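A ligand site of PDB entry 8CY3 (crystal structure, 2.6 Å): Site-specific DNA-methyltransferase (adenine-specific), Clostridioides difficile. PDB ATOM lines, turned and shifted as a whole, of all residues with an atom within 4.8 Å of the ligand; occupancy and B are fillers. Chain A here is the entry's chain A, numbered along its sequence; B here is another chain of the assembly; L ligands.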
ATOM      1  N   GLY A  29      -5.136  30.246  27.622  1.00  0.00           N
ATOM      2  CA  GLY A  29      -6.359  29.786  26.999  1.00  0.00           C
ATOM      3  C   GLY A  29      -7.291  30.904  26.566  1.00  0.00           C
ATOM      4  O   GLY A  29      -8.503  30.745  26.550  1.00  0.00           O
ATOM      5  N   ILE A  30      -6.709  32.050  26.213  1.00  0.00           N
ATOM      6  CA  ILE A  30      -7.453  33.216  25.751  1.00  0.00           C
ATOM      7  C   ILE A  30      -6.907  33.629  24.394  1.00  0.00           C
ATOM      8  O   ILE A  30      -5.699  33.859  24.247  1.00  0.00           O
ATOM      9  CB  ILE A  30      -7.381  34.377  26.752  1.00  0.00           C
ATOM     10  N   TYR A  31      -7.800  33.721  23.406  1.00  0.00           N
ATOM     11  CA  TYR A  31      -7.427  34.024  22.028  1.00  0.00           C
ATOM     12  C   TYR A  31      -8.005  35.376  21.630  1.00  0.00           C
ATOM     13  O   TYR A  31      -9.190  35.637  21.874  1.00  0.00           O
ATOM     14  CB  TYR A  31      -7.924  32.933  21.079  1.00  0.00           C
ATOM     15  CG  TYR A  31      -7.484  31.527  21.433  1.00  0.00           C
ATOM     16  CD1 TYR A  31      -8.227  30.744  22.298  1.00  0.00           C
ATOM     17  CD2 TYR A  31      -6.331  30.990  20.879  1.00  0.00           C
ATOM     18  CE1 TYR A  31      -7.831  29.458  22.619  1.00  0.00           C
ATOM     19  CE2 TYR A  31      -5.923  29.707  21.195  1.00  0.00           C
ATOM     20  CZ  TYR A  31      -6.684  28.944  22.070  1.00  0.00           C
ATOM     21  OH  TYR A  31      -6.284  27.671  22.391  1.00  0.00           O
ATOM     22  N   ILE A  62     -21.035  34.665  25.490  1.00  0.00           N
ATOM     23  CA  ILE A  62     -20.925  33.609  26.494  1.00  0.00           C
ATOM     24  C   ILE A  62     -19.510  33.072  26.642  1.00  0.00           C
ATOM     25  O   ILE A  62     -19.272  32.170  27.462  1.00  0.00           O
ATOM     26  CB  ILE A  62     -21.874  32.425  26.209  1.00  0.00           C
ATOM     27  CG1 ILE A  62     -21.605  31.784  24.842  1.00  0.00           C
ATOM     28  CG2 ILE A  62     -23.320  32.865  26.314  1.00  0.00           C
ATOM     29  CD1 ILE A  62     -22.519  30.606  24.529  1.00  0.00           C
ATOM     30  N   SER A  63     -18.544  33.590  25.874  1.00  0.00           N
ATOM     31  CA  SER A  63     -17.125  33.330  26.096  1.00  0.00           C
ATOM     32  C   SER A  63     -16.355  34.645  25.959  1.00  0.00           C
ATOM     33  O   SER A  63     -15.355  34.748  25.253  1.00  0.00           O
ATOM     34  CB  SER A  63     -16.601  32.263  25.135  1.00  0.00           C
ATOM     35  OG  SER A  63     -17.126  32.440  23.831  1.00  0.00           O
ATOM     36  N   GLY A  65     -14.279  36.464  27.479  1.00  0.00           N
ATOM     37  CA  GLY A  65     -12.863  36.679  27.740  1.00  0.00           C
ATOM     38  C   GLY A  65     -12.633  38.020  28.419  1.00  0.00           C
ATOM     39  O   GLY A  65     -13.297  38.372  29.403  1.00  0.00           O
ATOM     40  N   ALA A 114     -20.322  36.245  29.861  1.00  0.00           N
ATOM     41  CA  ALA A 114     -20.043  35.077  30.664  1.00  0.00           C
ATOM     42  C   ALA A 114     -18.715  34.477  30.230  1.00  0.00           C
ATOM     43  O   ALA A 114     -18.408  34.428  29.033  1.00  0.00           O
ATOM     44  CB  ALA A 114     -21.155  34.017  30.546  1.00  0.00           C
ATOM     45  N   ASP A 115     -17.915  34.044  31.209  1.00  0.00           N
ATOM     46  CA  ASP A 115     -16.656  33.383  30.907  1.00  0.00           C
ATOM     47  C   ASP A 115     -16.228  32.551  32.100  1.00  0.00           C
ATOM     48  O   ASP A 115     -16.647  32.794  33.237  1.00  0.00           O
ATOM     49  CB  ASP A 115     -15.569  34.404  30.532  1.00  0.00           C
ATOM     50  CG  ASP A 115     -14.391  33.762  29.823  1.00  0.00           C
ATOM     51  OD1 ASP A 115     -13.641  32.985  30.470  1.00  0.00           O
ATOM     52  OD2 ASP A 115     -14.216  34.001  28.611  1.00  0.00           O
ATOM     53  N   ILE A 116     -15.376  31.562  31.830  1.00  0.00           N
ATOM     54  CA  ILE A 116     -14.914  30.675  32.889  1.00  0.00           C
ATOM     55  C   ILE A 116     -13.701  31.242  33.628  1.00  0.00           C
ATOM     56  O   ILE A 116     -13.386  30.800  34.741  1.00  0.00           O
ATOM     57  CB  ILE A 116     -14.592  29.279  32.318  1.00  0.00           C
ATOM     58  CG1 ILE A 116     -14.605  28.219  33.428  1.00  0.00           C
ATOM     59  CG2 ILE A 116     -13.258  29.291  31.594  1.00  0.00           C
ATOM     60  CD1 ILE A 116     -15.936  28.082  34.140  1.00  0.00           C
ATOM     61  N   ASP A 117     -13.019  32.227  33.043  1.00  0.00           N
ATOM     62  CA  ASP A 117     -11.814  32.793  33.627  1.00  0.00           C
ATOM     63  C   ASP A 117     -12.179  33.972  34.520  1.00  0.00           C
ATOM     64  O   ASP A 117     -12.724  34.979  34.044  1.00  0.00           O
ATOM     65  CB  ASP A 117     -10.835  33.220  32.534  1.00  0.00           C
ATOM     66  CG  ASP A 117      -9.518  33.714  33.099  1.00  0.00           C
ATOM     67  OD1 ASP A 117      -9.180  33.333  34.240  1.00  0.00           O
ATOM     68  OD2 ASP A 117      -8.830  34.499  32.411  1.00  0.00           O
ATOM     69  N   CYS A 149     -18.643  31.655  35.020  1.00  0.00           N
ATOM     70  CA  CYS A 149     -19.337  30.371  35.056  1.00  0.00           C
ATOM     71  C   CYS A 149     -19.026  29.591  33.791  1.00  0.00           C
ATOM     72  O   CYS A 149     -18.379  30.089  32.860  1.00  0.00           O
ATOM     73  CB  CYS A 149     -20.846  30.565  35.199  1.00  0.00           C
ATOM     74  SG  CYS A 149     -21.618  31.317  33.734  1.00  0.00           S
ATOM     75  N   ASP A 150     -19.489  28.343  33.777  1.00  0.00           N
ATOM     76  CA  ASP A 150     -19.468  27.505  32.580  1.00  0.00           C
ATOM     77  C   ASP A 150     -20.768  27.768  31.822  1.00  0.00           C
ATOM     78  O   ASP A 150     -21.843  27.365  32.268  1.00  0.00           O
ATOM     79  CB  ASP A 150     -19.334  26.029  32.970  1.00  0.00           C
ATOM     80  CG  ASP A 150     -19.229  25.098  31.765  1.00  0.00           C
ATOM     81  OD1 ASP A 150     -19.689  25.459  30.664  1.00  0.00           O
ATOM     82  OD2 ASP A 150     -18.688  23.991  31.942  1.00  0.00           O
ATOM     83  N   SER A 151     -20.658  28.439  30.678  1.00  0.00           N
ATOM     84  CA  SER A 151     -21.840  28.804  29.902  1.00  0.00           C
ATOM     85  C   SER A 151     -22.644  27.588  29.460  1.00  0.00           C
ATOM     86  O   SER A 151     -23.850  27.707  29.218  1.00  0.00           O
ATOM     87  CB  SER A 151     -21.438  29.642  28.687  1.00  0.00           C
ATOM     88  OG  SER A 151     -20.793  30.838  29.078  1.00  0.00           O
ATOM     89  N   LEU A 152     -22.008  26.422  29.341  1.00  0.00           N
ATOM     90  CA  LEU A 152     -22.733  25.203  28.990  1.00  0.00           C
ATOM     91  C   LEU A 152     -23.487  24.597  30.157  1.00  0.00           C
ATOM     92  O   LEU A 152     -24.296  23.686  29.941  1.00  0.00           O
ATOM     93  CB  LEU A 152     -21.761  24.164  28.415  1.00  0.00           C
ATOM     94  CG  LEU A 152     -21.048  24.574  27.129  1.00  0.00           C
ATOM     95  CD1 LEU A 152     -20.277  23.402  26.543  1.00  0.00           C
ATOM     96  CD2 LEU A 152     -22.032  25.125  26.110  1.00  0.00           C
ATOM     97  N   ASN A 166     -16.524  34.608  20.215  1.00  0.00           N
ATOM     98  CA  ASN A 166     -15.614  33.592  19.682  1.00  0.00           C
ATOM     99  C   ASN A 166     -15.555  32.432  20.674  1.00  0.00           C
ATOM    100  O   ASN A 166     -14.807  32.500  21.671  1.00  0.00           O
ATOM    101  CB  ASN A 166     -14.235  34.179  19.434  1.00  0.00           C
ATOM    102  CG  ASN A 166     -13.229  33.148  18.946  1.00  0.00           C
ATOM    103  OD1 ASN A 166     -13.595  32.084  18.448  1.00  0.00           O
ATOM    104  ND2 ASN A 166     -11.949  33.460  19.092  1.00  0.00           N
ATOM    105  N   PRO A 167     -16.304  31.360  20.436  1.00  0.00           N
ATOM    106  CA  PRO A 167     -16.380  30.261  21.424  1.00  0.00           C
ATOM    107  C   PRO A 167     -15.062  29.507  21.494  1.00  0.00           C
ATOM    108  O   PRO A 167     -14.214  29.643  20.605  1.00  0.00           O
ATOM    109  CB  PRO A 167     -17.500  29.377  20.868  1.00  0.00           C
ATOM    110  CG  PRO A 167     -17.431  29.600  19.391  1.00  0.00           C
ATOM    111  CD  PRO A 167     -17.072  31.052  19.222  1.00  0.00           C
ATOM    112  N   PRO A 168     -14.843  28.723  22.550  1.00  0.00           N
ATOM    113  CA  PRO A 168     -13.645  27.896  22.623  1.00  0.00           C
ATOM    114  C   PRO A 168     -13.741  26.670  21.722  1.00  0.00           C
ATOM    115  O   PRO A 168     -14.803  26.049  21.609  1.00  0.00           O
ATOM    116  CB  PRO A 168     -13.577  27.501  24.099  1.00  0.00           C
ATOM    117  CG  PRO A 168     -14.996  27.497  24.533  1.00  0.00           C
ATOM    118  CD  PRO A 168     -15.655  28.628  23.788  1.00  0.00           C
ATOM    119  N   LEU A 175     -10.116  17.411  25.125  1.00  0.00           N
ATOM    120  CA  LEU A 175     -11.194  17.675  26.065  1.00  0.00           C
ATOM    121  C   LEU A 175     -11.173  16.650  27.188  1.00  0.00           C
ATOM    122  O   LEU A 175     -10.936  15.458  26.954  1.00  0.00           O
ATOM    123  CB  LEU A 175     -12.544  17.652  25.348  1.00  0.00           C
ATOM    124  CG  LEU A 175     -13.755  18.158  26.141  1.00  0.00           C
ATOM    125  CD1 LEU A 175     -13.463  19.504  26.761  1.00  0.00           C
ATOM    126  CD2 LEU A 175     -14.983  18.233  25.257  1.00  0.00           C
ATOM    127  N   GLU A 176     -11.402  17.125  28.407  1.00  0.00           N
ATOM    128  CA  GLU A 176     -11.391  16.235  29.572  1.00  0.00           C
ATOM    129  C   GLU A 176     -12.487  15.192  29.448  1.00  0.00           C
ATOM    130  O   GLU A 176     -13.632  15.505  29.082  1.00  0.00           O
ATOM    131  CB  GLU A 176     -11.557  17.059  30.852  1.00  0.00           C
ATOM    132  CG  GLU A 176     -11.303  16.286  32.134  1.00  0.00           C
ATOM    133  CD  GLU A 176     -11.492  17.130  33.376  1.00  0.00           C
ATOM    134  OE1 GLU A 176     -12.282  18.097  33.336  1.00  0.00           O
ATOM    135  OE2 GLU A 176     -10.841  16.822  34.402  1.00  0.00           O
ATOM    136  N   TYR A 179     -15.624  15.706  31.614  1.00  0.00           N
ATOM    137  CA  TYR A 179     -16.488  16.740  31.049  1.00  0.00           C
ATOM    138  C   TYR A 179     -17.201  16.235  29.793  1.00  0.00           C
ATOM    139  O   TYR A 179     -18.360  16.597  29.527  1.00  0.00           O
ATOM    140  CB  TYR A 179     -15.661  17.986  30.747  1.00  0.00           C
ATOM    141  CG  TYR A 179     -16.501  19.208  30.441  1.00  0.00           C
ATOM    142  CD1 TYR A 179     -16.914  20.052  31.453  1.00  0.00           C
ATOM    143  CD2 TYR A 179     -16.848  19.523  29.133  1.00  0.00           C
ATOM    144  CE1 TYR A 179     -17.670  21.166  31.189  1.00  0.00           C
ATOM    145  CE2 TYR A 179     -17.611  20.639  28.854  1.00  0.00           C
ATOM    146  CZ  TYR A 179     -18.016  21.459  29.885  1.00  0.00           C
ATOM    147  OH  TYR A 179     -18.772  22.581  29.609  1.00  0.00           O
ATOM    148  N   LEU A 197     -16.186  20.946  21.066  1.00  0.00           N
ATOM    149  CA  LEU A 197     -16.898  21.682  22.101  1.00  0.00           C
ATOM    150  C   LEU A 197     -17.730  22.824  21.524  1.00  0.00           C
ATOM    151  O   LEU A 197     -18.830  23.149  22.003  1.00  0.00           O
ATOM    152  CB  LEU A 197     -15.881  22.223  23.116  1.00  0.00           C
ATOM    153  CG  LEU A 197     -16.345  23.032  24.325  1.00  0.00           C
ATOM    154  CD1 LEU A 197     -17.120  22.143  25.258  1.00  0.00           C
ATOM    155  CD2 LEU A 197     -15.135  23.643  25.031  1.00  0.00           C
ATOM    156  N   PHE A 201     -21.405  24.937  21.956  1.00  0.00           N
ATOM    157  CA  PHE A 201     -21.625  26.386  22.066  1.00  0.00           C
ATOM    158  C   PHE A 201     -22.632  26.877  21.020  1.00  0.00           C
ATOM    159  O   PHE A 201     -23.471  27.739  21.317  1.00  0.00           O
ATOM    160  CB  PHE A 201     -20.313  27.152  21.973  1.00  0.00           C
ATOM    161  CG  PHE A 201     -19.654  27.365  23.291  1.00  0.00           C
ATOM    162  CD1 PHE A 201     -19.003  26.320  23.913  1.00  0.00           C
ATOM    163  CD2 PHE A 201     -19.707  28.593  23.934  1.00  0.00           C
ATOM    164  CE1 PHE A 201     -18.396  26.485  25.128  1.00  0.00           C
ATOM    165  CE2 PHE A 201     -19.101  28.766  25.170  1.00  0.00           C
ATOM    166  CZ  PHE A 201     -18.444  27.712  25.763  1.00  0.00           C
ATOM    167  P    DA B   8      -7.205  21.010  17.091  1.00  0.00           P
ATOM    168  OP1  DA B   8      -6.012  20.636  17.887  1.00  0.00           O
ATOM    169  OP2  DA B   8      -8.552  20.750  17.628  1.00  0.00           O
ATOM    170  O5'  DA B   8      -7.110  22.560  16.713  1.00  0.00           O
ATOM    171  C5'  DA B   8      -7.658  23.543  17.570  1.00  0.00           C
ATOM    172  C4'  DA B   8      -6.920  24.858  17.415  1.00  0.00           C
ATOM    173  O4'  DA B   8      -7.830  25.970  17.621  1.00  0.00           O
ATOM    174  C3'  DA B   8      -5.768  25.059  18.409  1.00  0.00           C
ATOM    175  O3'  DA B   8      -4.667  25.676  17.736  1.00  0.00           O
ATOM    176  C2'  DA B   8      -6.384  25.990  19.444  1.00  0.00           C
ATOM    177  C1'  DA B   8      -7.273  26.849  18.568  1.00  0.00           C
ATOM    178  N9   DA B   8      -8.366  27.491  19.289  1.00  0.00           N
ATOM    179  C8   DA B   8      -9.084  26.983  20.333  1.00  0.00           C
ATOM    180  N7   DA B   8     -10.017  27.798  20.769  1.00  0.00           N
ATOM    181  C5   DA B   8      -9.895  28.918  19.966  1.00  0.00           C
ATOM    182  C6   DA B   8     -10.600  30.133  19.923  1.00  0.00           C
ATOM    183  N6   DA B   8     -11.601  30.434  20.749  1.00  0.00           N
ATOM    184  N1   DA B   8     -10.222  31.034  18.985  1.00  0.00           N
ATOM    185  C2   DA B   8      -9.221  30.733  18.158  1.00  0.00           C
ATOM    186  N3   DA B   8      -8.494  29.619  18.105  1.00  0.00           N
ATOM    187  C4   DA B   8      -8.877  28.742  19.048  1.00  0.00           C
HETATM  188  N1  LIG L   1     -14.733  27.239  28.017  1.00  0.00           N
HETATM  189  C1  LIG L   1     -15.557  29.304  28.525  1.00  0.00           C
HETATM  190  C2  LIG L   1     -17.493  29.759  29.498  1.00  0.00           C
HETATM  191  N2  LIG L   1     -16.369  30.264  28.983  1.00  0.00           N
HETATM  192  C3  LIG L   1     -17.035  27.540  29.123  1.00  0.00           C
HETATM  193  O1  LIG L   1     -12.016  31.203  29.267  1.00  0.00           O
HETATM  194  C4  LIG L   1     -12.215  30.810  27.911  1.00  0.00           C
HETATM  195  C5  LIG L   1     -13.891  28.182  27.668  1.00  0.00           C
HETATM  196  C6  LIG L   1     -15.804  27.938  28.568  1.00  0.00           C
HETATM  197  N3  LIG L   1     -17.863  28.483  29.586  1.00  0.00           N
HETATM  198  C7  LIG L   1     -13.690  30.717  27.587  1.00  0.00           C
HETATM  199  C8  LIG L   1     -12.201  31.451  24.451  1.00  0.00           C
HETATM  200  O2  LIG L   1     -13.777  30.885  26.193  1.00  0.00           O
HETATM  201  C9  LIG L   1     -12.772  31.846  25.804  1.00  0.00           C
HETATM  202  N4  LIG L   1     -17.454  26.260  29.149  1.00  0.00           N
HETATM  203  N5  LIG L   1     -14.331  29.455  27.937  1.00  0.00           N
HETATM  204  C10 LIG L   1     -11.757  31.923  26.949  1.00  0.00           C
HETATM  205  O3  LIG L   1     -11.801  33.199  27.555  1.00  0.00           O
HETATM  206  C11 LIG L   1     -16.717  25.133  28.595  1.00  0.00           C
HETATM  207  C12 LIG L   1     -15.849  24.488  29.645  1.00  0.00           C
HETATM  208  C13 LIG L   1     -14.968  23.391  29.074  1.00  0.00           C
HETATM  209  C14 LIG L   1     -13.984  22.847  30.081  1.00  0.00           C
HETATM  210  C15 LIG L   1     -13.166  23.701  30.808  1.00  0.00           C
HETATM  211  C16 LIG L   1     -12.269  23.213  31.745  1.00  0.00           C
HETATM  212  C17 LIG L   1     -12.188  21.843  31.997  1.00  0.00           C
HETATM  213  C18 LIG L   1     -13.013  20.984  31.266  1.00  0.00           C
HETATM  214  C19 LIG L   1     -13.894  21.489  30.323  1.00  0.00           C
HETATM  215  N6  LIG L   1     -11.316  21.347  32.944  1.00  0.00           N
HETATM  216  O4  LIG L   1     -11.078  30.601  24.613  1.00  0.00           O
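Merely in contact with the ligand: Tyr 31, Ile 62, Ser 63, Gly 65, Cys 149, Asn 166, Pro 168, Tyr 179, Phe 201 and DA 8 of chain B. Within 4 Å of the ligand: Gly 29, Tyr 31, Ile 62, Ser 63, Gly 65, Asp 115, Ile 116, Cys 149, Asp 150, Ser 151, Asn 166, Pro 168, Glu 176, Tyr 179, Phe 201 and DA 8 of chain B. Along chain A the residues within 4 Å of the ligand span positions 29 to 201. The nearest printed residue that does not touch the ligand is Asp 117 (4.02 Å).
OD1 of Asp 150 is in hydrogen-bond range of N of Leu 152. N of Ser 63 is in hydrogen-bond range of O of Ala 114, at 3.3 Å. The backbone carbonyl oxygen (O) of Pro 167 lies close to N6 of DA 8 of chain B (2.7 Å). N of Ile 116 lies close to O of Cys 149, 3.5 Å away. N1 of DA 8 of chain B sits at hydrogen-bond distance from the side-chain amide nitrogen (ND2) of Asn 166 (3.0 Å). The backbone NH (N) of Asp 117 is in hydrogen-bond range of the side-chain carboxylate (OD1) of Asp 115 (2.8 Å). The side-chain hydroxyl of Ser 63 lies within hydrogen-bond range of the backbone carbonyl oxygen of Asn 166 (3.2 Å). The backbone NH of Cys 149 is in hydrogen-bond range of the backbone carbonyl oxygen of Asp 115 (2.9 Å).
The backbone NH (N) of Ser 151 lies within hydrogen-bond range of a nitrogen (N3) of the ligand (3.0 Å). The side-chain carboxylate of Asp 150 sits at hydrogen-bond distance from a nitrogen (N4) of the ligand (2.8 Å). An oxygen (O4) of the ligand lies within hydrogen-bond range of the backbone carbonyl oxygen (O) of Gly 29, 3.2 Å away. The backbone NH (N) of Ile 116 is in hydrogen-bond range of a nitrogen (N2) of the ligand, 3.3 Å away. The side-chain carboxylate (OE1) of Glu 176 sits at hydrogen-bond distance from a nitrogen (N6) of the ligand (3.4 Å). An oxygen (O1) of the ligand lies within hydrogen-bond range of the side-chain carboxylate (OD1) of Asp 115.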
